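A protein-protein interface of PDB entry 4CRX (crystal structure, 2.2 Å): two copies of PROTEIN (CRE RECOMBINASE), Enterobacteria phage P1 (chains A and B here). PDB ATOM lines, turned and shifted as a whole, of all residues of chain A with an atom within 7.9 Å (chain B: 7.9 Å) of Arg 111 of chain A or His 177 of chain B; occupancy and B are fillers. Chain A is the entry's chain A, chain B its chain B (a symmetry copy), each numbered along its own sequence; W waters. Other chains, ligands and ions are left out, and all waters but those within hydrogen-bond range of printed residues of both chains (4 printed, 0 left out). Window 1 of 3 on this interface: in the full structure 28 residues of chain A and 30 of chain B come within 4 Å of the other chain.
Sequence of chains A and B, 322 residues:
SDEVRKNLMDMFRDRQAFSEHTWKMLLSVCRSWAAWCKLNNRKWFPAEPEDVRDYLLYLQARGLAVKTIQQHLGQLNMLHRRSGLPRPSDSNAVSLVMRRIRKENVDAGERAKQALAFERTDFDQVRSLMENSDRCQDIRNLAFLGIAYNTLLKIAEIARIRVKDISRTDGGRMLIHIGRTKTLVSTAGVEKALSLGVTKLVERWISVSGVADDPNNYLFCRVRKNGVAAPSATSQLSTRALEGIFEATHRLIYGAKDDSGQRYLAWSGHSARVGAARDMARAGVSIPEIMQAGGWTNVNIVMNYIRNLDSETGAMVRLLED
The guanidinium group (NH2) of Arg 111 of chain A lies within hydrogen-bond range of a ring nitrogen (ND1) of His 177 of chain B. The side-chain carboxylate (OE2) of Glu 191 of chain B is in salt-bridge range of the guanidinium group (NH2) of Arg 111 of chain A, at 3.98 Å. N of Ala 112 of chain A lies within hydrogen-bond range of O of Thr 187 of chain B, 2.9 Å away. The guanidinium group (NH2) of Arg 307 of chain A lies within hydrogen-bond range of the backbone carbonyl oxygen (O) of Ala 188 of chain B (3.3 Å).
Water W1 lies within hydrogen-bond range of the side-chain carboxylate of Asp 165 of chain B (2.7 Å) and the guanidinium group of Arg 111 of chain A (2.8 Å). Water W2 lies within hydrogen-bond range of O of Ala 188 of chain B (2.9 Å), O of Ala 112 of chain A (3.0 Å), NH2 of Arg 307 of chain A (3.2 Å) and NE of Arg 111 of chain A (3.2 Å). Water W3 lies within hydrogen-bond range of OG1 of Thr 187 of chain B and OE2 of Glu 110 of chain A. Water W4 bridges the side-chain carboxylate of Asp 165 of chain B (3.2 Å) and the backbone carbonyl oxygen of Gly 109 of chain A (3.3 Å).
Printed residues of chain B that touch a printed residue of chain A: His 177, Arg 180, Thr 187, Ala 188 and Glu 191. Hydrophobic or aromatic side chains of chain B within 4 Å of the printed part of chain A: His 177. Among the printed residues, Asp or Glu carboxylates within 4 Å of a Lys or Arg side-chain nitrogen of the other chain: Arg 111 of chain A with Glu 191 of chain B.
The backbone carbonyl oxygen (O) of Asn 105 of chain A lies within hydrogen-bond range of the backbone NH (N) of Glu 110 of chain A, at 3.0 Å. The guanidinium group (NH2) of Arg 160 of chain B is in hydrogen-bond range of the backbone carbonyl oxygen (O) of Arg 180 of chain B (2.5 Å). The backbone NH of His 177 of chain B is in hydrogen-bond range of the backbone carbonyl oxygen of Asp 165 of chain B, at 3.0 Å. The backbone carbonyl oxygen of Ala 188 of chain B sits close to a ring nitrogen (NE2) of His 177 of chain B (3.5 Å). The side-chain carboxylate of Glu 191 of chain B is in hydrogen-bond range of a ring nitrogen (ND1) of His 177 of chain B, 3.1 Å away. The side-chain hydroxyl (OG) of Ser 186 of chain B lies close to the backbone NH (N) of Ala 188 of chain B, at 3.2 Å.
Of the printed residues of chain B, Arg 111 of chain A touches His 177 (3.0 Å), Thr 187 (3.2 Å) and Glu 191 (3.98 Å). His 177 of chain B touches just one residue of chain A: Arg 111. Printed residues of chain A within 4 Å of Thr 187 of chain B: Val 106 (3.9 Å), Glu 110 (3.9 Å), Arg 111 (3.2 Å) and Ala 112 (2.9 Å). Printed residues of chain B within 4 Å of Arg 307 of chain A: Ala 188 (3.3 Å) and Glu 191 (3.4 Å). Printed residues of chain A within 4 Å of Glu 191 of chain B: Arg 111 and Arg 307. Ile 161 of chain B touches none of the printed residues of chain A. Leu 175 of chain B touches none of the printed residues of chain A. The nearest printed residue of chain B that does not touch Arg 111 of chain A is Asp 165 of chain B (4.6 Å).
No position is printed for both chains. Of the 10 pairs that touch across the chains among the printed residues, none has its exchanged pair printed and touching as well.
Among the printed residues, pairs that only touch across the chains: Arg 111 of chain A with Thr 187 of chain B (3.2 Å), Arg 307 of chain A with Glu 191 of chain B (3.4 Å), Val 106 of chain A with Arg 180 of chain B (3.4 Å), Ala 112 of chain A with Ala 188 of chain B (3.8 Å), Glu 110 of chain A with Thr 187 of chain B (3.9 Å) and Val 106 of chain A with Thr 187 of chain B (3.9 Å).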
ATOM      1  N   ALA A  65     -15.358  18.189 -41.633  1.00  0.00           N
ATOM      2  CA  ALA A  65     -15.464  18.290 -40.184  1.00  0.00           C
ATOM      3  C   ALA A  65     -16.898  18.050 -39.724  1.00  0.00           C
ATOM      4  O   ALA A  65     -17.834  18.072 -40.526  1.00  0.00           O
ATOM      5  CB  ALA A  65     -14.997  19.669 -39.721  1.00  0.00           C
ATOM      6  N   VAL A  66     -17.060  17.814 -38.427  1.00  0.00           N
ATOM      7  CA  VAL A  66     -18.379  17.597 -37.855  1.00  0.00           C
ATOM      8  C   VAL A  66     -19.176  18.897 -37.992  1.00  0.00           C
ATOM      9  O   VAL A  66     -20.376  18.867 -38.252  1.00  0.00           O
ATOM     10  CB  VAL A  66     -18.273  17.172 -36.369  1.00  0.00           C
ATOM     11  CG1 VAL A  66     -19.594  17.390 -35.649  1.00  0.00           C
ATOM     12  CG2 VAL A  66     -17.876  15.711 -36.287  1.00  0.00           C
ATOM     13  N   ASN A 105     -15.774  10.764 -35.325  1.00  0.00           N
ATOM     14  CA  ASN A 105     -14.790  11.779 -35.673  1.00  0.00           C
ATOM     15  C   ASN A 105     -14.070  12.337 -34.456  1.00  0.00           C
ATOM     16  O   ASN A 105     -12.870  12.600 -34.506  1.00  0.00           O
ATOM     17  CB  ASN A 105     -15.454  12.909 -36.462  1.00  0.00           C
ATOM     18  CG  ASN A 105     -15.705  12.532 -37.909  1.00  0.00           C
ATOM     19  OD1 ASN A 105     -16.021  11.382 -38.214  1.00  0.00           O
ATOM     20  ND2 ASN A 105     -15.561  13.496 -38.809  1.00  0.00           N
ATOM     21  N   VAL A 106     -14.795  12.513 -33.359  1.00  0.00           N
ATOM     22  CA  VAL A 106     -14.184  13.029 -32.144  1.00  0.00           C
ATOM     23  C   VAL A 106     -13.230  11.980 -31.582  1.00  0.00           C
ATOM     24  O   VAL A 106     -12.140  12.302 -31.109  1.00  0.00           O
ATOM     25  CB  VAL A 106     -15.250  13.371 -31.091  1.00  0.00           C
ATOM     26  CG1 VAL A 106     -14.595  13.583 -29.736  1.00  0.00           C
ATOM     27  CG2 VAL A 106     -16.014  14.615 -31.522  1.00  0.00           C
ATOM     28  N   ALA A 108     -11.661   9.795 -33.271  1.00  0.00           N
ATOM     29  CA  ALA A 108     -10.516   9.644 -34.165  1.00  0.00           C
ATOM     30  C   ALA A 108      -9.615  10.856 -33.995  1.00  0.00           C
ATOM     31  O   ALA A 108      -8.629  11.028 -34.714  1.00  0.00           O
ATOM     32  CB  ALA A 108     -10.982   9.535 -35.604  1.00  0.00           C
ATOM     33  N   GLY A 109      -9.982  11.708 -33.043  1.00  0.00           N
ATOM     34  CA  GLY A 109      -9.199  12.895 -32.762  1.00  0.00           C
ATOM     35  C   GLY A 109      -9.420  14.095 -33.663  1.00  0.00           C
ATOM     36  O   GLY A 109      -8.459  14.675 -34.166  1.00  0.00           O
ATOM     37  N   GLU A 110     -10.673  14.476 -33.883  1.00  0.00           N
ATOM     38  CA  GLU A 110     -10.939  15.643 -34.712  1.00  0.00           C
ATOM     39  C   GLU A 110     -10.996  16.839 -33.777  1.00  0.00           C
ATOM     40  O   GLU A 110     -11.550  16.742 -32.682  1.00  0.00           O
ATOM     41  CB  GLU A 110     -12.274  15.512 -35.446  1.00  0.00           C
ATOM     42  CG  GLU A 110     -12.647  16.767 -36.225  1.00  0.00           C
ATOM     43  CD  GLU A 110     -13.946  16.627 -36.988  1.00  0.00           C
ATOM     44  OE1 GLU A 110     -13.962  15.916 -38.014  1.00  0.00           O
ATOM     45  OE2 GLU A 110     -14.954  17.230 -36.563  1.00  0.00           O
ATOM     46  N   ARG A 111     -10.420  17.963 -34.192  1.00  0.00           N
ATOM     47  CA  ARG A 111     -10.439  19.147 -33.347  1.00  0.00           C
ATOM     48  C   ARG A 111     -10.600  20.453 -34.103  1.00  0.00           C
ATOM     49  O   ARG A 111     -10.057  20.640 -35.194  1.00  0.00           O
ATOM     50  CB  ARG A 111      -9.182  19.222 -32.474  1.00  0.00           C
ATOM     51  CG  ARG A 111      -7.922  18.651 -33.093  1.00  0.00           C
ATOM     52  CD  ARG A 111      -6.880  18.376 -32.015  1.00  0.00           C
ATOM     53  NE  ARG A 111      -6.622  19.548 -31.178  1.00  0.00           N
ATOM     54  CZ  ARG A 111      -5.427  19.874 -30.694  1.00  0.00           C
ATOM     55  NH1 ARG A 111      -4.375  19.110 -30.951  1.00  0.00           N
ATOM     56  NH2 ARG A 111      -5.282  20.960 -29.947  1.00  0.00           N
ATOM     57  N   ALA A 112     -11.363  21.352 -33.495  1.00  0.00           N
ATOM     58  CA  ALA A 112     -11.624  22.667 -34.055  1.00  0.00           C
ATOM     59  C   ALA A 112     -10.338  23.474 -33.971  1.00  0.00           C
ATOM     60  O   ALA A 112      -9.538  23.274 -33.058  1.00  0.00           O
ATOM     61  CB  ALA A 112     -12.725  23.352 -33.255  1.00  0.00           C
ATOM     62  N   LYS A 113     -10.128  24.376 -34.922  1.00  0.00           N
ATOM     63  CA  LYS A 113      -8.935  25.213 -34.907  1.00  0.00           C
ATOM     64  C   LYS A 113      -9.312  26.653 -34.570  1.00  0.00           C
ATOM     65  O   LYS A 113     -10.456  26.945 -34.217  1.00  0.00           O
ATOM     66  CB  LYS A 113      -8.226  25.172 -36.268  1.00  0.00           C
ATOM     67  CG  LYS A 113      -8.393  23.865 -37.020  1.00  0.00           C
ATOM     68  CD  LYS A 113      -7.052  23.197 -37.285  1.00  0.00           C
ATOM     69  CE  LYS A 113      -6.484  23.591 -38.638  1.00  0.00           C
ATOM     70  NZ  LYS A 113      -5.218  22.864 -38.923  1.00  0.00           N
ATOM     71  N   GLN A 114      -8.333  27.545 -34.667  1.00  0.00           N
ATOM     72  CA  GLN A 114      -8.539  28.959 -34.392  1.00  0.00           C
ATOM     73  C   GLN A 114      -7.305  29.722 -34.869  1.00  0.00           C
ATOM     74  O   GLN A 114      -6.213  29.161 -34.951  1.00  0.00           O
ATOM     75  CB  GLN A 114      -8.774  29.183 -32.899  1.00  0.00           C
ATOM     76  CG  GLN A 114      -7.509  29.317 -32.097  1.00  0.00           C
ATOM     77  CD  GLN A 114      -7.708  28.938 -30.651  1.00  0.00           C
ATOM     78  OE1 GLN A 114      -6.757  28.905 -29.875  1.00  0.00           O
ATOM     79  NE2 GLN A 114      -8.950  28.650 -30.279  1.00  0.00           N
ATOM     80  N   ARG A 307      -5.797  29.191 -23.416  1.00  0.00           N
ATOM     81  CA  ARG A 307      -5.603  27.864 -22.843  1.00  0.00           C
ATOM     82  C   ARG A 307      -4.175  27.456 -22.474  1.00  0.00           C
ATOM     83  O   ARG A 307      -3.920  27.054 -21.340  1.00  0.00           O
ATOM     84  CB  ARG A 307      -6.185  26.814 -23.788  1.00  0.00           C
ATOM     85  CG  ARG A 307      -5.604  26.868 -25.189  1.00  0.00           C
ATOM     86  CD  ARG A 307      -5.582  25.492 -25.828  1.00  0.00           C
ATOM     87  NE  ARG A 307      -6.837  25.202 -26.514  1.00  0.00           N
ATOM     88  CZ  ARG A 307      -6.918  24.698 -27.741  1.00  0.00           C
ATOM     89  NH1 ARG A 307      -5.815  24.432 -28.427  1.00  0.00           N
ATOM     90  NH2 ARG A 307      -8.105  24.475 -28.288  1.00  0.00           N
ATOM     91  N   LEU B 153      -7.503  12.806 -15.048  1.00  0.00           N
ATOM     92  CA  LEU B 153      -8.111  12.183 -16.219  1.00  0.00           C
ATOM     93  C   LEU B 153      -8.431  10.730 -15.901  1.00  0.00           C
ATOM     94  O   LEU B 153      -7.753  10.108 -15.085  1.00  0.00           O
ATOM     95  CB  LEU B 153      -7.156  12.237 -17.417  1.00  0.00           C
ATOM     96  CG  LEU B 153      -6.927  13.588 -18.102  1.00  0.00           C
ATOM     97  CD1 LEU B 153      -5.726  13.475 -19.029  1.00  0.00           C
ATOM     98  CD2 LEU B 153      -8.164  14.017 -18.889  1.00  0.00           C
ATOM     99  N   GLU B 157      -9.185   8.036 -21.003  1.00  0.00           N
ATOM    100  CA  GLU B 157      -8.647   9.216 -21.671  1.00  0.00           C
ATOM    101  C   GLU B 157      -7.125   9.201 -21.702  1.00  0.00           C
ATOM    102  O   GLU B 157      -6.521   9.642 -22.677  1.00  0.00           O
ATOM    103  CB  GLU B 157      -9.146  10.477 -20.974  1.00  0.00           C
ATOM    104  CG  GLU B 157     -10.360  10.216 -20.116  1.00  0.00           C
ATOM    105  CD  GLU B 157     -11.093  11.472 -19.731  1.00  0.00           C
ATOM    106  OE1 GLU B 157     -11.804  12.032 -20.591  1.00  0.00           O
ATOM    107  OE2 GLU B 157     -10.956  11.894 -18.566  1.00  0.00           O
ATOM    108  N   ARG B 160      -5.882   7.003 -24.384  1.00  0.00           N
ATOM    109  CA  ARG B 160      -6.117   7.582 -25.705  1.00  0.00           C
ATOM    110  C   ARG B 160      -5.089   8.628 -26.135  1.00  0.00           C
ATOM    111  O   ARG B 160      -4.970   8.919 -27.324  1.00  0.00           O
ATOM    112  CB  ARG B 160      -7.507   8.219 -25.750  1.00  0.00           C
ATOM    113  CG  ARG B 160      -8.573   7.357 -26.395  1.00  0.00           C
ATOM    114  CD  ARG B 160      -9.799   8.183 -26.761  1.00  0.00           C
ATOM    115  NE  ARG B 160     -10.360   8.870 -25.600  1.00  0.00           N
ATOM    116  CZ  ARG B 160     -11.213   8.318 -24.743  1.00  0.00           C
ATOM    117  NH1 ARG B 160     -11.605   7.062 -24.904  1.00  0.00           N
ATOM    118  NH2 ARG B 160     -11.663   9.017 -23.711  1.00  0.00           N
ATOM    119  N   ILE B 161      -4.358   9.202 -25.181  1.00  0.00           N
ATOM    120  CA  ILE B 161      -3.367  10.229 -25.510  1.00  0.00           C
ATOM    121  C   ILE B 161      -2.351   9.783 -26.558  1.00  0.00           C
ATOM    122  O   ILE B 161      -1.758   8.709 -26.454  1.00  0.00           O
ATOM    123  CB  ILE B 161      -2.566  10.704 -24.266  1.00  0.00           C
ATOM    124  CG1 ILE B 161      -3.506  11.315 -23.223  1.00  0.00           C
ATOM    125  CG2 ILE B 161      -1.518  11.736 -24.693  1.00  0.00           C
ATOM    126  CD1 ILE B 161      -2.930  11.355 -21.817  1.00  0.00           C
ATOM    127  N   ARG B 162      -2.156  10.629 -27.565  1.00  0.00           N
ATOM    128  CA  ARG B 162      -1.201  10.359 -28.630  1.00  0.00           C
ATOM    129  C   ARG B 162      -0.033  11.313 -28.440  1.00  0.00           C
ATOM    130  O   ARG B 162      -0.200  12.411 -27.909  1.00  0.00           O
ATOM    131  CB  ARG B 162      -1.834  10.596 -30.004  1.00  0.00           C
ATOM    132  CG  ARG B 162      -2.838   9.537 -30.428  1.00  0.00           C
ATOM    133  CD  ARG B 162      -3.061   9.534 -31.937  1.00  0.00           C
ATOM    134  NE  ARG B 162      -2.860   8.204 -32.504  1.00  0.00           N
ATOM    135  CZ  ARG B 162      -3.844   7.386 -32.864  1.00  0.00           C
ATOM    136  NH1 ARG B 162      -5.108   7.755 -32.721  1.00  0.00           N
ATOM    137  NH2 ARG B 162      -3.562   6.187 -33.354  1.00  0.00           N
ATOM    138  N   LYS B 164       1.400  13.160 -30.430  1.00  0.00           N
ATOM    139  CA  LYS B 164       1.096  14.423 -31.095  1.00  0.00           C
ATOM    140  C   LYS B 164       0.158  15.336 -30.306  1.00  0.00           C
ATOM    141  O   LYS B 164       0.025  16.520 -30.619  1.00  0.00           O
ATOM    142  CB  LYS B 164       0.499  14.147 -32.479  1.00  0.00           C
ATOM    143  CG  LYS B 164      -0.740  13.272 -32.462  1.00  0.00           C
ATOM    144  CD  LYS B 164      -1.080  12.801 -33.862  1.00  0.00           C
ATOM    145  CE  LYS B 164      -2.478  13.230 -34.275  1.00  0.00           C
ATOM    146  NZ  LYS B 164      -3.207  12.140 -34.983  1.00  0.00           N
ATOM    147  N   ASP B 165      -0.486  14.784 -29.284  1.00  0.00           N
ATOM    148  CA  ASP B 165      -1.405  15.548 -28.444  1.00  0.00           C
ATOM    149  C   ASP B 165      -0.675  16.337 -27.361  1.00  0.00           C
ATOM    150  O   ASP B 165      -1.308  17.030 -26.564  1.00  0.00           O
ATOM    151  CB  ASP B 165      -2.407  14.611 -27.767  1.00  0.00           C
ATOM    152  CG  ASP B 165      -3.419  14.047 -28.732  1.00  0.00           C
ATOM    153  OD1 ASP B 165      -3.740  14.738 -29.721  1.00  0.00           O
ATOM    154  OD2 ASP B 165      -3.894  12.914 -28.505  1.00  0.00           O
ATOM    155  N   ILE B 166       0.652  16.235 -27.334  1.00  0.00           N
ATOM    156  CA  ILE B 166       1.453  16.925 -26.324  1.00  0.00           C
ATOM    157  C   ILE B 166       2.150  18.201 -26.789  1.00  0.00           C
ATOM    158  O   ILE B 166       2.856  18.207 -27.796  1.00  0.00           O
ATOM    159  CB  ILE B 166       2.538  15.993 -25.743  1.00  0.00           C
ATOM    160  CG1 ILE B 166       1.908  14.667 -25.313  1.00  0.00           C
ATOM    161  CG2 ILE B 166       3.245  16.686 -24.580  1.00  0.00           C
ATOM    162  CD1 ILE B 166       2.807  13.795 -24.467  1.00  0.00           C
ATOM    163  N   SER B 167       1.952  19.279 -26.038  1.00  0.00           N
ATOM    164  CA  SER B 167       2.581  20.555 -26.347  1.00  0.00           C
ATOM    165  C   SER B 167       3.302  21.010 -25.088  1.00  0.00           C
ATOM    166  O   SER B 167       3.388  20.264 -24.115  1.00  0.00           O
ATOM    167  CB  SER B 167       1.536  21.599 -26.766  1.00  0.00           C
ATOM    168  OG  SER B 167       0.275  21.355 -26.170  1.00  0.00           O
ATOM    169  N   MET B 174       4.608  20.713 -19.786  1.00  0.00           N
ATOM    170  CA  MET B 174       3.934  19.932 -20.812  1.00  0.00           C
ATOM    171  C   MET B 174       2.438  20.199 -20.841  1.00  0.00           C
ATOM    172  O   MET B 174       1.839  20.541 -19.822  1.00  0.00           O
ATOM    173  CB  MET B 174       4.167  18.447 -20.568  1.00  0.00           C
ATOM    174  CG  MET B 174       5.136  17.819 -21.531  1.00  0.00           C
ATOM    175  SD  MET B 174       5.189  16.042 -21.313  1.00  0.00           S
ATOM    176  CE  MET B 174       6.848  15.698 -21.866  1.00  0.00           C
ATOM    177  N   LEU B 175       1.838  20.026 -22.012  1.00  0.00           N
ATOM    178  CA  LEU B 175       0.411  20.238 -22.184  1.00  0.00           C
ATOM    179  C   LEU B 175      -0.202  19.047 -22.897  1.00  0.00           C
ATOM    180  O   LEU B 175       0.327  18.568 -23.898  1.00  0.00           O
ATOM    181  CB  LEU B 175       0.158  21.506 -22.994  1.00  0.00           C
ATOM    182  CG  LEU B 175       0.630  22.778 -22.297  1.00  0.00           C
ATOM    183  CD1 LEU B 175       0.658  23.923 -23.294  1.00  0.00           C
ATOM    184  CD2 LEU B 175      -0.292  23.086 -21.124  1.00  0.00           C
ATOM    185  N   ILE B 176      -1.321  18.564 -22.377  1.00  0.00           N
ATOM    186  CA  ILE B 176      -1.972  17.426 -22.994  1.00  0.00           C
ATOM    187  C   ILE B 176      -3.376  17.773 -23.454  1.00  0.00           C
ATOM    188  O   ILE B 176      -4.250  18.089 -22.648  1.00  0.00           O
ATOM    189  CB  ILE B 176      -2.035  16.224 -22.034  1.00  0.00           C
ATOM    190  CG1 ILE B 176      -0.638  15.903 -21.494  1.00  0.00           C
ATOM    191  CG2 ILE B 176      -2.593  15.018 -22.767  1.00  0.00           C
ATOM    192  CD1 ILE B 176      -0.602  14.727 -20.532  1.00  0.00           C
ATOM    193  N   HIS B 177      -3.581  17.713 -24.765  1.00  0.00           N
ATOM    194  CA  HIS B 177      -4.880  18.014 -25.344  1.00  0.00           C
ATOM    195  C   HIS B 177      -5.809  16.822 -25.201  1.00  0.00           C
ATOM    196  O   HIS B 177      -5.464  15.707 -25.586  1.00  0.00           O
ATOM    197  CB  HIS B 177      -4.752  18.363 -26.824  1.00  0.00           C
ATOM    198  CG  HIS B 177      -6.026  18.863 -27.422  1.00  0.00           C
ATOM    199  ND1 HIS B 177      -6.445  20.168 -27.287  1.00  0.00           N
ATOM    200  CD2 HIS B 177      -7.010  18.220 -28.095  1.00  0.00           C
ATOM    201  CE1 HIS B 177      -7.633  20.309 -27.848  1.00  0.00           C
ATOM    202  NE2 HIS B 177      -7.998  19.142 -28.346  1.00  0.00           N
ATOM    203  N   ILE B 178      -6.994  17.063 -24.653  1.00  0.00           N
ATOM    204  CA  ILE B 178      -7.972  16.004 -24.468  1.00  0.00           C
ATOM    205  C   ILE B 178      -9.237  16.308 -25.271  1.00  0.00           C
ATOM    206  O   ILE B 178      -9.781  17.411 -25.198  1.00  0.00           O
ATOM    207  CB  ILE B 178      -8.311  15.830 -22.959  1.00  0.00           C
ATOM    208  CG1 ILE B 178      -7.195  15.053 -22.261  1.00  0.00           C
ATOM    209  CG2 ILE B 178      -9.597  15.047 -22.782  1.00  0.00           C
ATOM    210  CD1 ILE B 178      -6.168  15.922 -21.602  1.00  0.00           C
ATOM    211  N   GLY B 179      -9.688  15.330 -26.053  1.00  0.00           N
ATOM    212  CA  GLY B 179     -10.885  15.509 -26.860  1.00  0.00           C
ATOM    213  C   GLY B 179     -12.043  14.621 -26.433  1.00  0.00           C
ATOM    214  O   GLY B 179     -12.957  15.055 -25.730  1.00  0.00           O
ATOM    215  N   ARG B 180     -12.290  13.612 -26.490  1.00  0.00           N
ATOM    216  CA  ARG B 180     -13.422  12.830 -25.979  1.00  0.00           C
ATOM    217  C   ARG B 180     -13.089  12.183 -24.634  1.00  0.00           C
ATOM    218  O   ARG B 180     -12.189  11.335 -24.539  1.00  0.00           O
ATOM    219  CB  ARG B 180     -13.783  11.720 -26.965  1.00  0.00           C
ATOM    220  CG  ARG B 180     -15.022  10.929 -26.540  1.00  0.00           C
ATOM    221  CD  ARG B 180     -15.276   9.701 -27.415  1.00  0.00           C
ATOM    222  NE  ARG B 180     -14.086   8.854 -27.576  1.00  0.00           N
ATOM    223  CZ  ARG B 180     -14.101   7.517 -27.490  1.00  0.00           C
ATOM    224  NH1 ARG B 180     -15.239   6.854 -27.242  1.00  0.00           N
ATOM    225  NH2 ARG B 180     -13.016   6.745 -27.637  1.00  0.00           N
ATOM    226  N   SER B 186     -18.147  22.153 -28.286  1.00  0.00           N
ATOM    227  CA  SER B 186     -17.559  21.937 -29.605  1.00  0.00           C
ATOM    228  C   SER B 186     -16.308  21.059 -29.545  1.00  0.00           C
ATOM    229  O   SER B 186     -15.879  20.643 -28.467  1.00  0.00           O
ATOM    230  CB  SER B 186     -17.217  23.278 -30.261  1.00  0.00           C
ATOM    231  OG  SER B 186     -15.938  23.739 -29.860  1.00  0.00           O
ATOM    232  N   THR B 187     -15.730  20.790 -30.714  1.00  0.00           N
ATOM    233  CA  THR B 187     -14.536  19.955 -30.830  1.00  0.00           C
ATOM    234  C   THR B 187     -13.233  20.692 -30.517  1.00  0.00           C
ATOM    235  O   THR B 187     -12.153  20.247 -30.912  1.00  0.00           O
ATOM    236  CB  THR B 187     -14.413  19.345 -32.248  1.00  0.00           C
ATOM    237  OG1 THR B 187     -14.461  20.393 -33.225  1.00  0.00           O
ATOM    238  CG2 THR B 187     -15.544  18.357 -32.509  1.00  0.00           C
ATOM    239  N   ALA B 188     -13.336  21.816 -29.812  1.00  0.00           N
ATOM    240  CA  ALA B 188     -12.160  22.599 -29.438  1.00  0.00           C
ATOM    241  C   ALA B 188     -11.343  21.824 -28.410  1.00  0.00           C
ATOM    242  O   ALA B 188     -10.114  21.897 -28.395  1.00  0.00           O
ATOM    243  CB  ALA B 188     -12.585  23.945 -28.864  1.00  0.00           C
ATOM    244  N   GLY B 189     -12.040  21.088 -27.549  1.00  0.00           N
ATOM    245  CA  GLY B 189     -11.379  20.286 -26.534  1.00  0.00           C
ATOM    246  C   GLY B 189     -10.762  21.064 -25.390  1.00  0.00           C
ATOM    247  O   GLY B 189     -11.049  22.246 -25.198  1.00  0.00           O
ATOM    248  N   VAL B 190      -9.900  20.395 -24.631  1.00  0.00           N
ATOM    249  CA  VAL B 190      -9.240  21.012 -23.488  1.00  0.00           C
ATOM    250  C   VAL B 190      -7.751  20.676 -23.431  1.00  0.00           C
ATOM    251  O   VAL B 190      -7.286  19.756 -24.104  1.00  0.00           O
ATOM    252  CB  VAL B 190      -9.909  20.557 -22.165  1.00  0.00           C
ATOM    253  CG1 VAL B 190      -9.392  19.177 -21.758  1.00  0.00           C
ATOM    254  CG2 VAL B 190      -9.649  21.580 -21.072  1.00  0.00           C
ATOM    255  N   GLU B 191      -7.009  21.435 -22.630  1.00  0.00           N
ATOM    256  CA  GLU B 191      -5.574  21.215 -22.458  1.00  0.00           C
ATOM    257  C   GLU B 191      -5.275  21.002 -20.973  1.00  0.00           C
ATOM    258  O   GLU B 191      -5.659  21.814 -20.133  1.00  0.00           O
ATOM    259  CB  GLU B 191      -4.775  22.423 -22.973  1.00  0.00           C
ATOM    260  CG  GLU B 191      -4.695  22.547 -24.493  1.00  0.00           C
ATOM    261  CD  GLU B 191      -3.589  21.705 -25.115  1.00  0.00           C
ATOM    262  OE1 GLU B 191      -2.597  21.389 -24.423  1.00  0.00           O
ATOM    263  OE2 GLU B 191      -3.716  21.360 -26.309  1.00  0.00           O
ATOM    264  N   LYS B 192      -4.603  19.905 -20.645  1.00  0.00           N
ATOM    265  CA  LYS B 192      -4.254  19.630 -19.260  1.00  0.00           C
ATOM    266  C   LYS B 192      -2.763  19.891 -19.088  1.00  0.00           C
ATOM    267  O   LYS B 192      -1.932  19.326 -19.799  1.00  0.00           O
ATOM    268  CB  LYS B 192      -4.608  18.188 -18.894  1.00  0.00           C
ATOM    269  CG  LYS B 192      -6.081  17.867 -19.092  1.00  0.00           C
ATOM    270  CD  LYS B 192      -6.818  17.779 -17.770  1.00  0.00           C
ATOM    271  CE  LYS B 192      -6.943  19.142 -17.117  1.00  0.00           C
ATOM    272  NZ  LYS B 192      -7.958  19.139 -16.030  1.00  0.00           N
ATOM    273  N   ALA B 193      -2.437  20.770 -18.149  1.00  0.00           N
ATOM    274  CA  ALA B 193      -1.053  21.136 -17.890  1.00  0.00           C
ATOM    275  C   ALA B 193      -0.435  20.283 -16.792  1.00  0.00           C
ATOM    276  O   ALA B 193      -1.085  19.968 -15.798  1.00  0.00           O
ATOM    277  CB  ALA B 193      -0.980  22.604 -17.509  1.00  0.00           C
HETATM  278  O   HOH W   1      -3.801  16.525 -31.711  1.00  0.00           O
HETATM  279  O   HOH W   2      -8.266  22.260 -30.554  1.00  0.00           O
HETATM  280  O   HOH W   3     -16.130  19.846 -35.512  1.00  0.00           O
HETATM  281  O   HOH W   4      -6.139  15.044 -31.854  1.00  0.00           O
